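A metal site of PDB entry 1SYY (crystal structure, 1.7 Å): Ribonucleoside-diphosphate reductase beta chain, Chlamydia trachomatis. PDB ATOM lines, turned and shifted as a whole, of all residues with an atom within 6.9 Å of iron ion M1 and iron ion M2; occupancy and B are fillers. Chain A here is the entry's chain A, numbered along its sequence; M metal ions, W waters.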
ATOM      1  N   PHE A  85     -22.375   9.902  23.759  1.00  0.00           N
ATOM      2  CA  PHE A  85     -23.677  10.580  23.574  1.00  0.00           C
ATOM      3  C   PHE A  85     -24.727  10.167  24.584  1.00  0.00           C
ATOM      4  O   PHE A  85     -25.573  10.981  24.931  1.00  0.00           O
ATOM      5  CB  PHE A  85     -24.233  10.317  22.149  1.00  0.00           C
ATOM      6  CG  PHE A  85     -23.676  11.242  21.083  1.00  0.00           C
ATOM      7  CD1 PHE A  85     -22.467  10.956  20.466  1.00  0.00           C
ATOM      8  CD2 PHE A  85     -24.370  12.369  20.662  1.00  0.00           C
ATOM      9  CE1 PHE A  85     -21.921  11.743  19.465  1.00  0.00           C
ATOM     10  CE2 PHE A  85     -23.835  13.168  19.634  1.00  0.00           C
ATOM     11  CZ  PHE A  85     -22.592  12.834  19.033  1.00  0.00           C
ATOM     12  N   ALA A  88     -24.312  12.434  27.471  1.00  0.00           N
ATOM     13  CA  ALA A  88     -24.171  13.863  27.208  1.00  0.00           C
ATOM     14  C   ALA A  88     -25.489  14.485  26.886  1.00  0.00           C
ATOM     15  O   ALA A  88     -25.674  15.688  27.146  1.00  0.00           O
ATOM     16  CB  ALA A  88     -23.199  14.150  25.997  1.00  0.00           C
ATOM     17  N   GLU A  89     -26.405  13.730  26.288  1.00  0.00           N
ATOM     18  CA  GLU A  89     -27.711  14.311  26.007  1.00  0.00           C
ATOM     19  C   GLU A  89     -28.356  14.678  27.312  1.00  0.00           C
ATOM     20  O   GLU A  89     -29.006  15.768  27.352  1.00  0.00           O
ATOM     21  CB  GLU A  89     -28.677  13.318  25.294  1.00  0.00           C
ATOM     22  CG  GLU A  89     -28.028  12.743  24.013  1.00  0.00           C
ATOM     23  CD  GLU A  89     -27.942  13.763  22.881  1.00  0.00           C
ATOM     24  OE1 GLU A  89     -28.447  14.911  23.003  1.00  0.00           O
ATOM     25  OE2 GLU A  89     -27.396  13.438  21.825  1.00  0.00           O
ATOM     26  N   VAL A  92     -26.887  17.967  28.678  1.00  0.00           N
ATOM     27  CA  VAL A  92     -27.433  19.156  28.002  1.00  0.00           C
ATOM     28  C   VAL A  92     -28.877  19.455  28.457  1.00  0.00           C
ATOM     29  O   VAL A  92     -29.204  20.602  28.805  1.00  0.00           O
ATOM     30  CB  VAL A  92     -27.414  18.947  26.416  1.00  0.00           C
ATOM     31  CG1 VAL A  92     -27.967  20.249  25.703  1.00  0.00           C
ATOM     32  CG2 VAL A  92     -25.914  18.823  26.000  1.00  0.00           C
ATOM     33  N   ILE A  96     -30.271  22.790  30.415  1.00  0.00           N
ATOM     34  CA  ILE A  96     -31.331  23.758  29.937  1.00  0.00           C
ATOM     35  C   ILE A  96     -32.309  24.043  31.029  1.00  0.00           C
ATOM     36  O   ILE A  96     -32.717  25.184  31.246  1.00  0.00           O
ATOM     37  CB  ILE A  96     -32.110  23.043  28.766  1.00  0.00           C
ATOM     38  CG1 ILE A  96     -31.263  22.960  27.515  1.00  0.00           C
ATOM     39  CG2 ILE A  96     -33.414  23.919  28.431  1.00  0.00           C
ATOM     40  CD1 ILE A  96     -31.787  21.973  26.487  1.00  0.00           C
ATOM     41  N   GLN A 116     -36.444  22.320  23.095  1.00  0.00           N
ATOM     42  CA  GLN A 116     -35.061  21.800  23.035  1.00  0.00           C
ATOM     43  C   GLN A 116     -34.872  20.735  24.101  1.00  0.00           C
ATOM     44  O   GLN A 116     -34.297  19.674  23.791  1.00  0.00           O
ATOM     45  CB  GLN A 116     -34.053  22.929  23.240  1.00  0.00           C
ATOM     46  CG  GLN A 116     -32.627  22.436  22.906  1.00  0.00           C
ATOM     47  CD  GLN A 116     -31.502  23.368  23.360  1.00  0.00           C
ATOM     48  OE1 GLN A 116     -30.289  22.925  23.427  1.00  0.00           O
ATOM     49  NE2 GLN A 116     -31.849  24.587  23.715  1.00  0.00           N
ATOM     50  N   GLU A 119     -36.419  17.616  23.039  1.00  0.00           N
ATOM     51  CA  GLU A 119     -35.634  16.896  21.998  1.00  0.00           C
ATOM     52  C   GLU A 119     -34.454  16.188  22.633  1.00  0.00           C
ATOM     53  O   GLU A 119     -34.037  15.145  22.123  1.00  0.00           O
ATOM     54  CB  GLU A 119     -35.147  17.887  20.966  1.00  0.00           C
ATOM     55  CG  GLU A 119     -36.406  18.313  20.062  1.00  0.00           C
ATOM     56  CD  GLU A 119     -36.099  19.459  19.082  1.00  0.00           C
ATOM     57  OE1 GLU A 119     -35.026  20.106  19.119  1.00  0.00           O
ATOM     58  OE2 GLU A 119     -36.957  19.684  18.234  1.00  0.00           O
ATOM     59  N   GLU A 120     -33.843  16.755  23.683  1.00  0.00           N
ATOM     60  CA  GLU A 120     -32.705  16.015  24.277  1.00  0.00           C
ATOM     61  C   GLU A 120     -33.226  14.726  24.941  1.00  0.00           C
ATOM     62  O   GLU A 120     -32.488  13.721  24.973  1.00  0.00           O
ATOM     63  CB  GLU A 120     -31.985  16.867  25.339  1.00  0.00           C
ATOM     64  CG  GLU A 120     -31.444  18.233  24.841  1.00  0.00           C
ATOM     65  CD  GLU A 120     -30.545  18.202  23.643  1.00  0.00           C
ATOM     66  OE1 GLU A 120     -30.245  17.085  23.157  1.00  0.00           O
ATOM     67  OE2 GLU A 120     -30.130  19.334  23.184  1.00  0.00           O
ATOM     68  N   ALA A 121     -34.444  14.732  25.471  1.00  0.00           N
ATOM     69  CA  ALA A 121     -35.036  13.480  26.013  1.00  0.00           C
ATOM     70  C   ALA A 121     -35.202  12.458  24.851  1.00  0.00           C
ATOM     71  O   ALA A 121     -34.939  11.250  25.028  1.00  0.00           O
ATOM     72  CB  ALA A 121     -36.428  13.810  26.704  1.00  0.00           C
ATOM     73  N   HIS A 123     -33.334  12.372  22.236  1.00  0.00           N
ATOM     74  CA  HIS A 123     -31.985  11.866  21.911  1.00  0.00           C
ATOM     75  C   HIS A 123     -31.568  10.818  22.921  1.00  0.00           C
ATOM     76  O   HIS A 123     -30.933   9.826  22.549  1.00  0.00           O
ATOM     77  CB  HIS A 123     -30.983  13.040  21.908  1.00  0.00           C
ATOM     78  CG  HIS A 123     -31.306  14.035  20.828  1.00  0.00           C
ATOM     79  ND1 HIS A 123     -30.622  15.263  20.666  1.00  0.00           N
ATOM     80  CD2 HIS A 123     -32.297  13.997  19.883  1.00  0.00           C
ATOM     81  CE1 HIS A 123     -31.222  15.909  19.684  1.00  0.00           C
ATOM     82  NE2 HIS A 123     -32.231  15.185  19.201  1.00  0.00           N
ATOM     83  N   THR A 124     -31.880  11.020  24.203  1.00  0.00           N
ATOM     84  CA  THR A 124     -31.475   9.946  25.181  1.00  0.00           C
ATOM     85  C   THR A 124     -32.167   8.641  24.853  1.00  0.00           C
ATOM     86  O   THR A 124     -31.541   7.546  24.922  1.00  0.00           O
ATOM     87  CB  THR A 124     -31.902  10.386  26.578  1.00  0.00           C
ATOM     88  OG1 THR A 124     -31.156  11.578  26.936  1.00  0.00           O
ATOM     89  CG2 THR A 124     -31.613   9.283  27.702  1.00  0.00           C
ATOM     90  N   PHE A 127     -30.419   6.597  22.241  1.00  0.00           N
ATOM     91  CA  PHE A 127     -29.300   5.794  22.677  1.00  0.00           C
ATOM     92  C   PHE A 127     -29.734   4.531  23.451  1.00  0.00           C
ATOM     93  O   PHE A 127     -29.095   3.489  23.307  1.00  0.00           O
ATOM     94  CB  PHE A 127     -28.270   6.656  23.426  1.00  0.00           C
ATOM     95  CG  PHE A 127     -27.637   7.639  22.483  1.00  0.00           C
ATOM     96  CD1 PHE A 127     -26.795   7.167  21.411  1.00  0.00           C
ATOM     97  CD2 PHE A 127     -28.058   8.915  22.459  1.00  0.00           C
ATOM     98  CE1 PHE A 127     -26.470   8.010  20.375  1.00  0.00           C
ATOM     99  CE2 PHE A 127     -27.727   9.763  21.435  1.00  0.00           C
ATOM    100  CZ  PHE A 127     -26.941   9.324  20.373  1.00  0.00           C
ATOM    101  N   TYR A 188     -22.299  25.029  26.710  1.00  0.00           N
ATOM    102  CA  TYR A 188     -23.259  24.008  26.265  1.00  0.00           C
ATOM    103  C   TYR A 188     -23.627  24.152  24.781  1.00  0.00           C
ATOM    104  O   TYR A 188     -23.628  23.166  24.046  1.00  0.00           O
ATOM    105  CB  TYR A 188     -24.510  23.991  27.156  1.00  0.00           C
ATOM    106  CG  TYR A 188     -24.224  23.225  28.431  1.00  0.00           C
ATOM    107  CD1 TYR A 188     -24.503  21.831  28.519  1.00  0.00           C
ATOM    108  CD2 TYR A 188     -23.624  23.863  29.511  1.00  0.00           C
ATOM    109  CE1 TYR A 188     -24.225  21.155  29.676  1.00  0.00           C
ATOM    110  CE2 TYR A 188     -23.269  23.111  30.670  1.00  0.00           C
ATOM    111  CZ  TYR A 188     -23.594  21.797  30.713  1.00  0.00           C
ATOM    112  OH  TYR A 188     -23.232  21.073  31.881  1.00  0.00           O
ATOM    113  N   TYR A 189     -23.952  25.363  24.341  1.00  0.00           N
ATOM    114  CA  TYR A 189     -24.370  25.480  22.928  1.00  0.00           C
ATOM    115  C   TYR A 189     -23.220  25.432  21.980  1.00  0.00           C
ATOM    116  O   TYR A 189     -23.260  24.713  20.992  1.00  0.00           O
ATOM    117  CB  TYR A 189     -25.096  26.850  22.701  1.00  0.00           C
ATOM    118  CG  TYR A 189     -26.516  26.794  23.194  1.00  0.00           C
ATOM    119  CD1 TYR A 189     -27.489  26.041  22.493  1.00  0.00           C
ATOM    120  CD2 TYR A 189     -26.871  27.461  24.367  1.00  0.00           C
ATOM    121  CE1 TYR A 189     -28.822  26.016  22.989  1.00  0.00           C
ATOM    122  CE2 TYR A 189     -28.182  27.407  24.884  1.00  0.00           C
ATOM    123  CZ  TYR A 189     -29.139  26.694  24.174  1.00  0.00           C
ATOM    124  OH  TYR A 189     -30.396  26.653  24.727  1.00  0.00           O
ATOM    125  N   GLU A 193     -22.689  21.141  22.166  1.00  0.00           N
ATOM    126  CA  GLU A 193     -23.496  20.857  20.991  1.00  0.00           C
ATOM    127  C   GLU A 193     -22.832  21.203  19.707  1.00  0.00           C
ATOM    128  O   GLU A 193     -22.965  20.508  18.719  1.00  0.00           O
ATOM    129  CB  GLU A 193     -24.848  21.620  21.086  1.00  0.00           C
ATOM    130  CG  GLU A 193     -25.646  20.997  22.306  1.00  0.00           C
ATOM    131  CD  GLU A 193     -26.966  21.737  22.646  1.00  0.00           C
ATOM    132  OE1 GLU A 193     -26.974  22.880  23.128  1.00  0.00           O
ATOM    133  OE2 GLU A 193     -28.003  21.167  22.485  1.00  0.00           O
ATOM    134  N   PHE A 197     -20.310  17.408  19.744  1.00  0.00           N
ATOM    135  CA  PHE A 197     -21.296  16.481  19.059  1.00  0.00           C
ATOM    136  C   PHE A 197     -21.042  16.414  17.575  1.00  0.00           C
ATOM    137  O   PHE A 197     -21.112  15.339  16.976  1.00  0.00           O
ATOM    138  CB  PHE A 197     -22.703  16.944  19.244  1.00  0.00           C
ATOM    139  CG  PHE A 197     -23.235  16.787  20.654  1.00  0.00           C
ATOM    140  CD1 PHE A 197     -22.565  16.066  21.614  1.00  0.00           C
ATOM    141  CD2 PHE A 197     -24.506  17.275  20.986  1.00  0.00           C
ATOM    142  CE1 PHE A 197     -23.124  15.834  22.834  1.00  0.00           C
ATOM    143  CE2 PHE A 197     -25.058  17.033  22.199  1.00  0.00           C
ATOM    144  CZ  PHE A 197     -24.373  16.315  23.142  1.00  0.00           C
ATOM    145  N   PHE A 201     -20.724  13.221  15.026  1.00  0.00           N
ATOM    146  CA  PHE A 201     -21.615  13.067  13.851  1.00  0.00           C
ATOM    147  C   PHE A 201     -20.821  12.684  12.638  1.00  0.00           C
ATOM    148  O   PHE A 201     -21.267  11.866  11.848  1.00  0.00           O
ATOM    149  CB  PHE A 201     -22.331  14.433  13.501  1.00  0.00           C
ATOM    150  CG  PHE A 201     -23.277  14.930  14.558  1.00  0.00           C
ATOM    151  CD1 PHE A 201     -24.013  14.074  15.349  1.00  0.00           C
ATOM    152  CD2 PHE A 201     -23.493  16.283  14.707  1.00  0.00           C
ATOM    153  CE1 PHE A 201     -24.947  14.558  16.295  1.00  0.00           C
ATOM    154  CE2 PHE A 201     -24.460  16.785  15.651  1.00  0.00           C
ATOM    155  CZ  PHE A 201     -25.164  15.919  16.432  1.00  0.00           C
ATOM    156  N   ILE A 223     -30.753  13.503  14.709  1.00  0.00           N
ATOM    157  CA  ILE A 223     -30.165  14.293  15.822  1.00  0.00           C
ATOM    158  C   ILE A 223     -29.435  15.517  15.263  1.00  0.00           C
ATOM    159  O   ILE A 223     -29.577  16.621  15.801  1.00  0.00           O
ATOM    160  CB  ILE A 223     -29.198  13.440  16.690  1.00  0.00           C
ATOM    161  CG1 ILE A 223     -30.009  12.354  17.313  1.00  0.00           C
ATOM    162  CG2 ILE A 223     -28.423  14.273  17.667  1.00  0.00           C
ATOM    163  CD1 ILE A 223     -29.133  11.246  18.034  1.00  0.00           C
ATOM    164  N   ASP A 226     -31.798  18.282  14.463  1.00  0.00           N
ATOM    165  CA  ASP A 226     -32.175  19.023  15.695  1.00  0.00           C
ATOM    166  C   ASP A 226     -31.007  19.904  16.180  1.00  0.00           C
ATOM    167  O   ASP A 226     -31.214  21.057  16.502  1.00  0.00           O
ATOM    168  CB  ASP A 226     -32.543  18.092  16.864  1.00  0.00           C
ATOM    169  CG  ASP A 226     -33.769  17.239  16.590  1.00  0.00           C
ATOM    170  OD1 ASP A 226     -34.662  17.669  15.846  1.00  0.00           O
ATOM    171  OD2 ASP A 226     -33.841  16.133  17.209  1.00  0.00           O
ATOM    172  N   GLU A 227     -29.796  19.351  16.269  1.00  0.00           N
ATOM    173  CA  GLU A 227     -28.633  20.080  16.833  1.00  0.00           C
ATOM    174  C   GLU A 227     -28.349  21.353  16.073  1.00  0.00           C
ATOM    175  O   GLU A 227     -27.840  22.348  16.641  1.00  0.00           O
ATOM    176  CB  GLU A 227     -27.378  19.199  16.772  1.00  0.00           C
ATOM    177  CG  GLU A 227     -26.392  19.661  17.774  1.00  0.00           C
ATOM    178  CD  GLU A 227     -26.964  19.183  19.123  1.00  0.00           C
ATOM    179  OE1 GLU A 227     -26.795  17.982  19.375  1.00  0.00           O
ATOM    180  OE2 GLU A 227     -27.624  19.957  19.881  1.00  0.00           O
ATOM    181  N   HIS A 230     -30.563  23.741  17.611  1.00  0.00           N
ATOM    182  CA  HIS A 230     -30.109  24.072  18.965  1.00  0.00           C
ATOM    183  C   HIS A 230     -28.945  25.098  18.968  1.00  0.00           C
ATOM    184  O   HIS A 230     -28.936  26.061  19.728  1.00  0.00           O
ATOM    185  CB  HIS A 230     -29.617  22.812  19.685  1.00  0.00           C
ATOM    186  CG  HIS A 230     -30.685  21.773  19.883  1.00  0.00           C
ATOM    187  ND1 HIS A 230     -30.457  20.595  20.584  1.00  0.00           N
ATOM    188  CD2 HIS A 230     -31.969  21.745  19.509  1.00  0.00           C
ATOM    189  CE1 HIS A 230     -31.575  19.882  20.593  1.00  0.00           C
ATOM    190  NE2 HIS A 230     -32.511  20.557  19.944  1.00  0.00           N
ATOM    191  N   LEU A 231     -27.970  24.839  18.104  1.00  0.00           N
ATOM    192  CA  LEU A 231     -26.795  25.704  18.002  1.00  0.00           C
ATOM    193  C   LEU A 231     -27.224  27.096  17.529  1.00  0.00           C
ATOM    194  O   LEU A 231     -26.730  28.088  18.072  1.00  0.00           O
ATOM    195  CB  LEU A 231     -25.848  25.074  17.002  1.00  0.00           C
ATOM    196  CG  LEU A 231     -24.648  25.951  16.642  1.00  0.00           C
ATOM    197  CD1 LEU A 231     -23.771  26.257  17.859  1.00  0.00           C
ATOM    198  CD2 LEU A 231     -23.836  25.177  15.563  1.00  0.00           C
HETATM  199 FE    FE M   1     -28.972  16.280  21.764  1.00  0.00          FE
HETATM  200 FE    FE M   2     -28.835  19.610  21.560  1.00  0.00          FE
HETATM  201  O   HOH W   1     -27.538  15.611  20.459  1.00  0.00           O
HETATM  202  O   HOH W   2     -27.659  17.941  22.418  1.00  0.00           O
HETATM  203  O   HOH W   3     -29.083  17.844  20.413  1.00  0.00           O
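The backbone NH (N) of Glu 193 lies within hydrogen-bond range of the backbone carbonyl oxygen (O) of Tyr 188, at 2.9 Å. NE2 of His 123 sits close to O of Glu 119 (3.4 Å). A ring nitrogen (NE2) of His 123 is in hydrogen-bond range of the side-chain carboxylate (OD2) of Asp 226, 2.7 Å away. O of Glu 120 sits at hydrogen-bond distance from OG1 of Thr 124 (3.2 Å). The side-chain carboxylate (OE1) of Glu 119 sits at hydrogen-bond distance from a ring nitrogen (NE2) of His 230, 2.7 Å away. OE1 of Glu 193 lies close to OE1 of Gln 116.
Within 4 Å of iron ion M1: Glu 89, Glu 120, His 123 and Glu 227. Along chain A the residues within 4 Å of iron ion M1 span positions 89 to 227. The nearest printed residue that does not touch iron ion M1 is Phe 197 (4.01 Å).
Four residues have an atom within 4 Å of iron ion M2: Glu 120, Glu 193, Glu 227 and His 230. The nearest printed residue that does not touch iron ion M2 is Gln 116 (4.1 Å).
Iron ion M1 is bound by OE1 of Glu 89, water W1, OE1 of Glu 120, water W3, water W2 and ND1 of His 123. Iron ion M1 has six donor atoms within binding distance.
Iron ion M2 is bound by OE2 of Glu 193, OE2 of Glu 120, OE2 of Glu 227, water W3, ND1 of His 230 and water W2.
Water W1 bridges OE2 of Glu 89 and OE1 of Glu 227.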
